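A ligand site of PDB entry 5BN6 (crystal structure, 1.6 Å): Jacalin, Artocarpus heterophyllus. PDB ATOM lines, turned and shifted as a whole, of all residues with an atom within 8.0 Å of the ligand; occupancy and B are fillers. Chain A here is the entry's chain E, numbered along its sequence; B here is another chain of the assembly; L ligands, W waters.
An oxygen (O4) of the ligand lies within hydrogen-bond range of the side-chain carboxylate (OD1) of Asp 130, 2.6 Å away.
An oxygen (O4) of the ligand sits at hydrogen-bond distance from the backbone NH of Gly 6 (2.9 Å).
O of Trp 128 lies within hydrogen-bond range of O6 of the ligand (3.1 Å).
The backbone NH of Trp 128 lies within hydrogen-bond range of an oxygen (O6) of the ligand (2.9 Å).
N of Tyr 127 lies within hydrogen-bond range of O5 of the ligand, at 2.9 Å.
O of Asp 130 sits at hydrogen-bond distance from N of Ala 17 of chain B (2.8 Å).
OG of Ser 51 lies close to O of Gly 126 (3.4 Å).
The backbone carbonyl oxygen (O) of Tyr 127 lies within hydrogen-bond range of the side-chain hydroxyl (OG) of Ser 51 (2.6 Å).
The side-chain carboxylate (OD2) of Asp 130 is in hydrogen-bond range of the backbone NH (N) of Ile 125, 3.4 Å away.
The side-chain hydroxyl (OG) of Ser 124 is in hydrogen-bond range of the side-chain carboxylate (OD2) of Asp 130 (2.7 Å).
The backbone NH (N) of Phe 52 sits at hydrogen-bond distance from the backbone carbonyl oxygen (O) of Gly 126, 2.8 Å away.
OD2 of Asp 130 sits at hydrogen-bond distance from N of Gly 126.
Merely in contact with the ligand: Phe 52 (3.1 Å), Tyr 83 (3.6 Å), Val 85 (3.98 Å) and Gly 126 (3.5 Å).
Hydrophobic or aromatic side chains within 4 Å of the ligand: Phe 52, Tyr 83, Val 85, Tyr 127 and Trp 128.
Within 4 Å of the ligand: Gly 6, Phe 52, Tyr 83, Val 85, Gly 126, Tyr 127, Trp 128 and Asp 130.
The nearest printed residue that does not touch the ligand is Ile 125 (4.8 Å).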
ATOM      1  N   GLY A   6      -7.276 -11.646  20.711  1.00  0.00           N
ATOM      2  CA  GLY A   6      -8.411 -11.224  21.513  1.00  0.00           C
ATOM      3  C   GLY A   6      -9.273 -10.207  20.779  1.00  0.00           C
ATOM      4  O   GLY A   6      -8.985  -9.830  19.647  1.00  0.00           O
ATOM      5  N   LYS A   7     -10.349  -9.782  21.429  1.00  0.00           N
ATOM      6  CA  LYS A   7     -11.259  -8.812  20.847  1.00  0.00           C
ATOM      7  C   LYS A   7     -10.820  -7.382  21.159  1.00  0.00           C
ATOM      8  O   LYS A   7     -10.690  -7.015  22.316  1.00  0.00           O
ATOM      9  CB  LYS A   7     -12.684  -9.029  21.345  1.00  0.00           C
ATOM     10  CG  LYS A   7     -13.699  -8.096  20.712  1.00  0.00           C
ATOM     11  CD  LYS A   7     -15.110  -8.581  20.988  1.00  0.00           C
ATOM     12  CE  LYS A   7     -15.814  -7.711  22.012  1.00  0.00           C
ATOM     13  NZ  LYS A   7     -16.331  -6.446  21.408  1.00  0.00           N
ATOM     14  N   ALA A  29      -3.644 -13.085  35.151  1.00  0.00           N
ATOM     15  CA  ALA A  29      -3.537 -11.734  34.618  1.00  0.00           C
ATOM     16  C   ALA A  29      -4.841 -10.968  34.762  1.00  0.00           C
ATOM     17  O   ALA A  29      -5.812 -11.473  35.330  1.00  0.00           O
ATOM     18  CB  ALA A  29      -3.103 -11.789  33.151  1.00  0.00           C
ATOM     19  N   ILE A  30      -4.862  -9.748  34.218  1.00  0.00           N
ATOM     20  CA  ILE A  30      -6.085  -8.961  34.149  1.00  0.00           C
ATOM     21  C   ILE A  30      -7.100  -9.609  33.220  1.00  0.00           C
ATOM     22  O   ILE A  30      -6.736 -10.114  32.156  1.00  0.00           O
ATOM     23  CB  ILE A  30      -5.792  -7.510  33.659  1.00  0.00           C
ATOM     24  CG1 ILE A  30      -4.791  -6.833  34.593  1.00  0.00           C
ATOM     25  CG2 ILE A  30      -7.070  -6.705  33.586  1.00  0.00           C
ATOM     26  CD1 ILE A  30      -5.322  -6.613  36.007  1.00  0.00           C
ATOM     27  N   SER A  51     -13.444 -10.677  29.349  1.00  0.00           N
ATOM     28  CA  SER A  51     -12.653 -11.850  29.024  1.00  0.00           C
ATOM     29  C   SER A  51     -13.504 -12.960  28.427  1.00  0.00           C
ATOM     30  O   SER A  51     -14.713 -13.039  28.714  1.00  0.00           O
ATOM     31  CB  SER A  51     -11.931 -12.371  30.279  1.00  0.00           C
ATOM     32  OG  SER A  51     -11.477 -13.699  30.092  1.00  0.00           O
ATOM     33  N   PHE A  52     -12.880 -13.827  27.636  1.00  0.00           N
ATOM     34  CA  PHE A  52     -13.529 -15.001  27.078  1.00  0.00           C
ATOM     35  C   PHE A  52     -13.863 -16.024  28.171  1.00  0.00           C
ATOM     36  O   PHE A  52     -14.694 -16.911  27.960  1.00  0.00           O
ATOM     37  CB  PHE A  52     -12.640 -15.673  26.010  1.00  0.00           C
ATOM     38  CG  PHE A  52     -12.373 -14.834  24.788  1.00  0.00           C
ATOM     39  CD1 PHE A  52     -13.111 -13.695  24.517  1.00  0.00           C
ATOM     40  CD2 PHE A  52     -11.395 -15.220  23.882  1.00  0.00           C
ATOM     41  CE1 PHE A  52     -12.853 -12.936  23.382  1.00  0.00           C
ATOM     42  CE2 PHE A  52     -11.138 -14.477  22.752  1.00  0.00           C
ATOM     43  CZ  PHE A  52     -11.867 -13.329  22.493  1.00  0.00           C
ATOM     44  N   ILE A  53     -13.213 -15.902  29.328  1.00  0.00           N
ATOM     45  CA  ILE A  53     -13.391 -16.884  30.395  1.00  0.00           C
ATOM     46  C   ILE A  53     -13.786 -16.221  31.712  1.00  0.00           C
ATOM     47  O   ILE A  53     -13.838 -14.989  31.815  1.00  0.00           O
ATOM     48  CB  ILE A  53     -12.118 -17.729  30.616  1.00  0.00           C
ATOM     49  CG1 ILE A  53     -10.926 -16.830  30.990  1.00  0.00           C
ATOM     50  CG2 ILE A  53     -11.818 -18.539  29.359  1.00  0.00           C
ATOM     51  CD1 ILE A  53      -9.639 -17.613  31.324  1.00  0.00           C
ATOM     52  N   VAL A  80       1.382 -15.622  29.566  1.00  0.00           N
ATOM     53  CA  VAL A  80       0.450 -16.539  30.214  1.00  0.00           C
ATOM     54  C   VAL A  80      -0.060 -17.468  29.127  1.00  0.00           C
ATOM     55  O   VAL A  80      -0.622 -17.014  28.136  1.00  0.00           O
ATOM     56  CB  VAL A  80      -0.726 -15.804  30.895  1.00  0.00           C
ATOM     57  CG1 VAL A  80      -1.683 -16.802  31.497  1.00  0.00           C
ATOM     58  CG2 VAL A  80      -0.217 -14.844  31.950  1.00  0.00           C
ATOM     59  N   SER A  81       0.178 -18.765  29.302  1.00  0.00           N
ATOM     60  CA  SER A  81      -0.168 -19.775  28.297  1.00  0.00           C
ATOM     61  C   SER A  81       0.360 -19.433  26.908  1.00  0.00           C
ATOM     62  O   SER A  81      -0.320 -19.674  25.912  1.00  0.00           O
ATOM     63  CB  SER A  81      -1.678 -19.967  28.236  1.00  0.00           C
ATOM     64  OG  SER A  81      -2.194 -20.362  29.493  1.00  0.00           O
ATOM     65  N   GLY A  82       1.556 -18.868  26.851  1.00  0.00           N
ATOM     66  CA  GLY A  82       2.173 -18.537  25.583  1.00  0.00           C
ATOM     67  C   GLY A  82       1.839 -17.160  25.040  1.00  0.00           C
ATOM     68  O   GLY A  82       2.455 -16.704  24.080  1.00  0.00           O
ATOM     69  N   TYR A  83       0.858 -16.498  25.642  1.00  0.00           N
ATOM     70  CA  TYR A  83       0.408 -15.171  25.187  1.00  0.00           C
ATOM     71  C   TYR A  83       0.984 -14.049  26.034  1.00  0.00           C
ATOM     72  O   TYR A  83       0.938 -14.109  27.252  1.00  0.00           O
ATOM     73  CB  TYR A  83      -1.124 -15.062  25.225  1.00  0.00           C
ATOM     74  CG  TYR A  83      -1.851 -16.055  24.368  1.00  0.00           C
ATOM     75  CD1 TYR A  83      -2.002 -15.853  23.003  1.00  0.00           C
ATOM     76  CD2 TYR A  83      -2.408 -17.197  24.925  1.00  0.00           C
ATOM     77  CE1 TYR A  83      -2.672 -16.774  22.209  1.00  0.00           C
ATOM     78  CE2 TYR A  83      -3.078 -18.113  24.144  1.00  0.00           C
ATOM     79  CZ  TYR A  83      -3.208 -17.906  22.784  1.00  0.00           C
ATOM     80  OH  TYR A  83      -3.876 -18.838  22.031  1.00  0.00           O
ATOM     81  N   VAL A  84       1.494 -13.012  25.373  1.00  0.00           N
ATOM     82  CA  VAL A  84       1.884 -11.793  26.073  1.00  0.00           C
ATOM     83  C   VAL A  84       0.635 -11.032  26.470  1.00  0.00           C
ATOM     84  O   VAL A  84      -0.189 -10.679  25.619  1.00  0.00           O
ATOM     85  CB  VAL A  84       2.807 -10.900  25.209  1.00  0.00           C
ATOM     86  CG1 VAL A  84       3.131  -9.606  25.945  1.00  0.00           C
ATOM     87  CG2 VAL A  84       4.088 -11.662  24.855  1.00  0.00           C
ATOM     88  N   VAL A  85       0.481 -10.788  27.767  1.00  0.00           N
ATOM     89  CA  VAL A  85      -0.719 -10.139  28.283  1.00  0.00           C
ATOM     90  C   VAL A  85      -0.355  -9.144  29.390  1.00  0.00           C
ATOM     91  O   VAL A  85       0.795  -9.077  29.834  1.00  0.00           O
ATOM     92  CB  VAL A  85      -1.724 -11.170  28.846  1.00  0.00           C
ATOM     93  CG1 VAL A  85      -2.241 -12.096  27.728  1.00  0.00           C
ATOM     94  CG2 VAL A  85      -1.082 -11.996  29.939  1.00  0.00           C
ATOM     95  N   VAL A  86      -1.352  -8.366  29.827  1.00  0.00           N
ATOM     96  CA  VAL A  86      -1.164  -7.416  30.909  1.00  0.00           C
ATOM     97  C   VAL A  86      -1.435  -8.171  32.215  1.00  0.00           C
ATOM     98  O   VAL A  86      -2.583  -8.496  32.502  1.00  0.00           O
ATOM     99  CB  VAL A  86      -2.114  -6.212  30.780  1.00  0.00           C
ATOM    100  CG1 VAL A  86      -1.927  -5.227  31.947  1.00  0.00           C
ATOM    101  CG2 VAL A  86      -1.884  -5.498  29.452  1.00  0.00           C
ATOM    102  N   SER A 124      -7.325  -4.653  23.949  1.00  0.00           N
ATOM    103  CA  SER A 124      -7.841  -5.923  23.457  1.00  0.00           C
ATOM    104  C   SER A 124      -7.902  -6.918  24.607  1.00  0.00           C
ATOM    105  O   SER A 124      -7.014  -6.935  25.454  1.00  0.00           O
ATOM    106  CB  SER A 124      -6.942  -6.461  22.336  1.00  0.00           C
ATOM    107  OG  SER A 124      -7.272  -7.794  22.017  1.00  0.00           O
ATOM    108  N   ILE A 125      -8.952  -7.734  24.626  1.00  0.00           N
ATOM    109  CA  ILE A 125      -9.086  -8.771  25.650  1.00  0.00           C
ATOM    110  C   ILE A 125      -9.479 -10.091  25.015  1.00  0.00           C
ATOM    111  O   ILE A 125     -10.451 -10.162  24.261  1.00  0.00           O
ATOM    112  CB  ILE A 125     -10.159  -8.406  26.716  1.00  0.00           C
ATOM    113  CG1 ILE A 125      -9.910  -7.016  27.280  1.00  0.00           C
ATOM    114  CG2 ILE A 125     -10.151  -9.410  27.845  1.00  0.00           C
ATOM    115  CD1 ILE A 125     -10.942  -6.576  28.289  1.00  0.00           C
ATOM    116  N   GLY A 126      -8.732 -11.142  25.330  1.00  0.00           N
ATOM    117  CA  GLY A 126      -9.093 -12.492  24.935  1.00  0.00           C
ATOM    118  C   GLY A 126      -9.401 -13.250  26.220  1.00  0.00           C
ATOM    119  O   GLY A 126     -10.332 -12.895  26.942  1.00  0.00           O
ATOM    120  N   TYR A 127      -8.611 -14.282  26.513  1.00  0.00           N
ATOM    121  CA  TYR A 127      -8.639 -14.873  27.852  1.00  0.00           C
ATOM    122  C   TYR A 127      -8.279 -13.800  28.865  1.00  0.00           C
ATOM    123  O   TYR A 127      -8.874 -13.703  29.941  1.00  0.00           O
ATOM    124  CB  TYR A 127      -7.654 -16.042  27.969  1.00  0.00           C
ATOM    125  CG  TYR A 127      -7.986 -17.266  27.149  1.00  0.00           C
ATOM    126  CD1 TYR A 127      -9.300 -17.636  26.918  1.00  0.00           C
ATOM    127  CD2 TYR A 127      -6.965 -18.058  26.627  1.00  0.00           C
ATOM    128  CE1 TYR A 127      -9.598 -18.765  26.170  1.00  0.00           C
ATOM    129  CE2 TYR A 127      -7.260 -19.191  25.887  1.00  0.00           C
ATOM    130  CZ  TYR A 127      -8.572 -19.540  25.664  1.00  0.00           C
ATOM    131  OH  TYR A 127      -8.861 -20.660  24.927  1.00  0.00           O
ATOM    132  N   TRP A 128      -7.292 -12.975  28.516  1.00  0.00           N
ATOM    133  CA  TRP A 128      -6.808 -11.908  29.392  1.00  0.00           C
ATOM    134  C   TRP A 128      -6.671 -10.599  28.619  1.00  0.00           C
ATOM    135  O   TRP A 128      -6.774 -10.591  27.385  1.00  0.00           O
ATOM    136  CB  TRP A 128      -5.463 -12.312  30.021  1.00  0.00           C
ATOM    137  CG  TRP A 128      -5.616 -13.629  30.693  1.00  0.00           C
ATOM    138  CD1 TRP A 128      -6.267 -13.863  31.877  1.00  0.00           C
ATOM    139  CD2 TRP A 128      -5.184 -14.904  30.212  1.00  0.00           C
ATOM    140  NE1 TRP A 128      -6.233 -15.210  32.165  1.00  0.00           N
ATOM    141  CE2 TRP A 128      -5.581 -15.866  31.159  1.00  0.00           C
ATOM    142  CE3 TRP A 128      -4.478 -15.324  29.071  1.00  0.00           C
ATOM    143  CZ2 TRP A 128      -5.308 -17.229  31.011  1.00  0.00           C
ATOM    144  CZ3 TRP A 128      -4.205 -16.687  28.924  1.00  0.00           C
ATOM    145  CH2 TRP A 128      -4.619 -17.613  29.881  1.00  0.00           C
ATOM    146  N   LEU A 129      -6.475  -9.506  29.338  1.00  0.00           N
ATOM    147  CA  LEU A 129      -6.167  -8.236  28.685  1.00  0.00           C
ATOM    148  C   LEU A 129      -4.850  -8.363  27.904  1.00  0.00           C
ATOM    149  O   LEU A 129      -3.790  -8.526  28.489  1.00  0.00           O
ATOM    150  CB  LEU A 129      -6.082  -7.090  29.718  1.00  0.00           C
ATOM    151  CG  LEU A 129      -5.797  -5.687  29.177  1.00  0.00           C
ATOM    152  CD1 LEU A 129      -6.944  -5.204  28.321  1.00  0.00           C
ATOM    153  CD2 LEU A 129      -5.571  -4.680  30.314  1.00  0.00           C
ATOM    154  N   ASP A 130      -4.935  -8.316  26.575  1.00  0.00           N
ATOM    155  CA  ASP A 130      -3.766  -8.521  25.720  1.00  0.00           C
ATOM    156  C   ASP A 130      -2.852  -7.311  25.772  1.00  0.00           C
ATOM    157  O   ASP A 130      -1.626  -7.438  25.869  1.00  0.00           O
ATOM    158  CB  ASP A 130      -4.180  -8.798  24.257  1.00  0.00           C
ATOM    159  CG  ASP A 130      -5.165  -9.945  24.133  1.00  0.00           C
ATOM    160  OD1 ASP A 130      -4.814 -11.086  24.476  1.00  0.00           O
ATOM    161  OD2 ASP A 130      -6.294  -9.698  23.649  1.00  0.00           O
ATOM    162  N   TYR A 131      -3.468  -6.142  25.660  1.00  0.00           N
ATOM    163  CA  TYR A 131      -2.746  -4.888  25.673  1.00  0.00           C
ATOM    164  C   TYR A 131      -3.722  -3.763  25.930  1.00  0.00           C
ATOM    165  O   TYR A 131      -4.939  -3.947  25.805  1.00  0.00           O
ATOM    166  CB  TYR A 131      -2.000  -4.653  24.344  1.00  0.00           C
ATOM    167  CG  TYR A 131      -2.878  -4.723  23.108  1.00  0.00           C
ATOM    168  CD1 TYR A 131      -3.645  -3.632  22.690  1.00  0.00           C
ATOM    169  CD2 TYR A 131      -2.920  -5.874  22.322  1.00  0.00           C
ATOM    170  CE1 TYR A 131      -4.446  -3.701  21.549  1.00  0.00           C
ATOM    171  CE2 TYR A 131      -3.709  -5.947  21.174  1.00  0.00           C
ATOM    172  CZ  TYR A 131      -4.467  -4.854  20.800  1.00  0.00           C
ATOM    173  OH  TYR A 131      -5.249  -4.934  19.670  1.00  0.00           O
ATOM    174  N   ALA B  17       0.783  -7.207  24.454  1.00  0.00           N
ATOM    175  CA  ALA B  17       1.139  -7.878  23.208  1.00  0.00           C
ATOM    176  C   ALA B  17       1.272  -6.822  22.110  1.00  0.00           C
ATOM    177  O   ALA B  17       0.581  -5.810  22.128  1.00  0.00           O
ATOM    178  CB  ALA B  17       0.093  -8.919  22.840  1.00  0.00           C
HETATM  179  C1  LIG L   1      -7.226 -16.166  23.565  1.00  0.00           C
HETATM  180  C2  LIG L   1      -7.209 -15.483  22.187  1.00  0.00           C
HETATM  181  C3  LIG L   1      -5.801 -14.951  21.850  1.00  0.00           C
HETATM  182  C4  LIG L   1      -5.297 -14.033  22.994  1.00  0.00           C
HETATM  183  C5  LIG L   1      -5.367 -14.869  24.284  1.00  0.00           C
HETATM  184  C6  LIG L   1      -4.860 -14.182  25.574  1.00  0.00           C
HETATM  185  O1  LIG L   1      -8.549 -16.504  23.922  1.00  0.00           O
HETATM  186  O2  LIG L   1      -7.568 -16.389  21.161  1.00  0.00           O
HETATM  187  O3  LIG L   1      -5.838 -14.196  20.666  1.00  0.00           O
HETATM  188  O4  LIG L   1      -6.136 -12.863  23.082  1.00  0.00           O
HETATM  189  O5  LIG L   1      -6.713 -15.285  24.549  1.00  0.00           O
HETATM  190  O6  LIG L   1      -5.761 -13.189  26.024  1.00  0.00           O
HETATM  191  O   HOH W   1      -3.166 -13.264  19.744  1.00  0.00           O
HETATM  192  O   HOH W   2      -6.013 -15.501  18.149  1.00  0.00           O
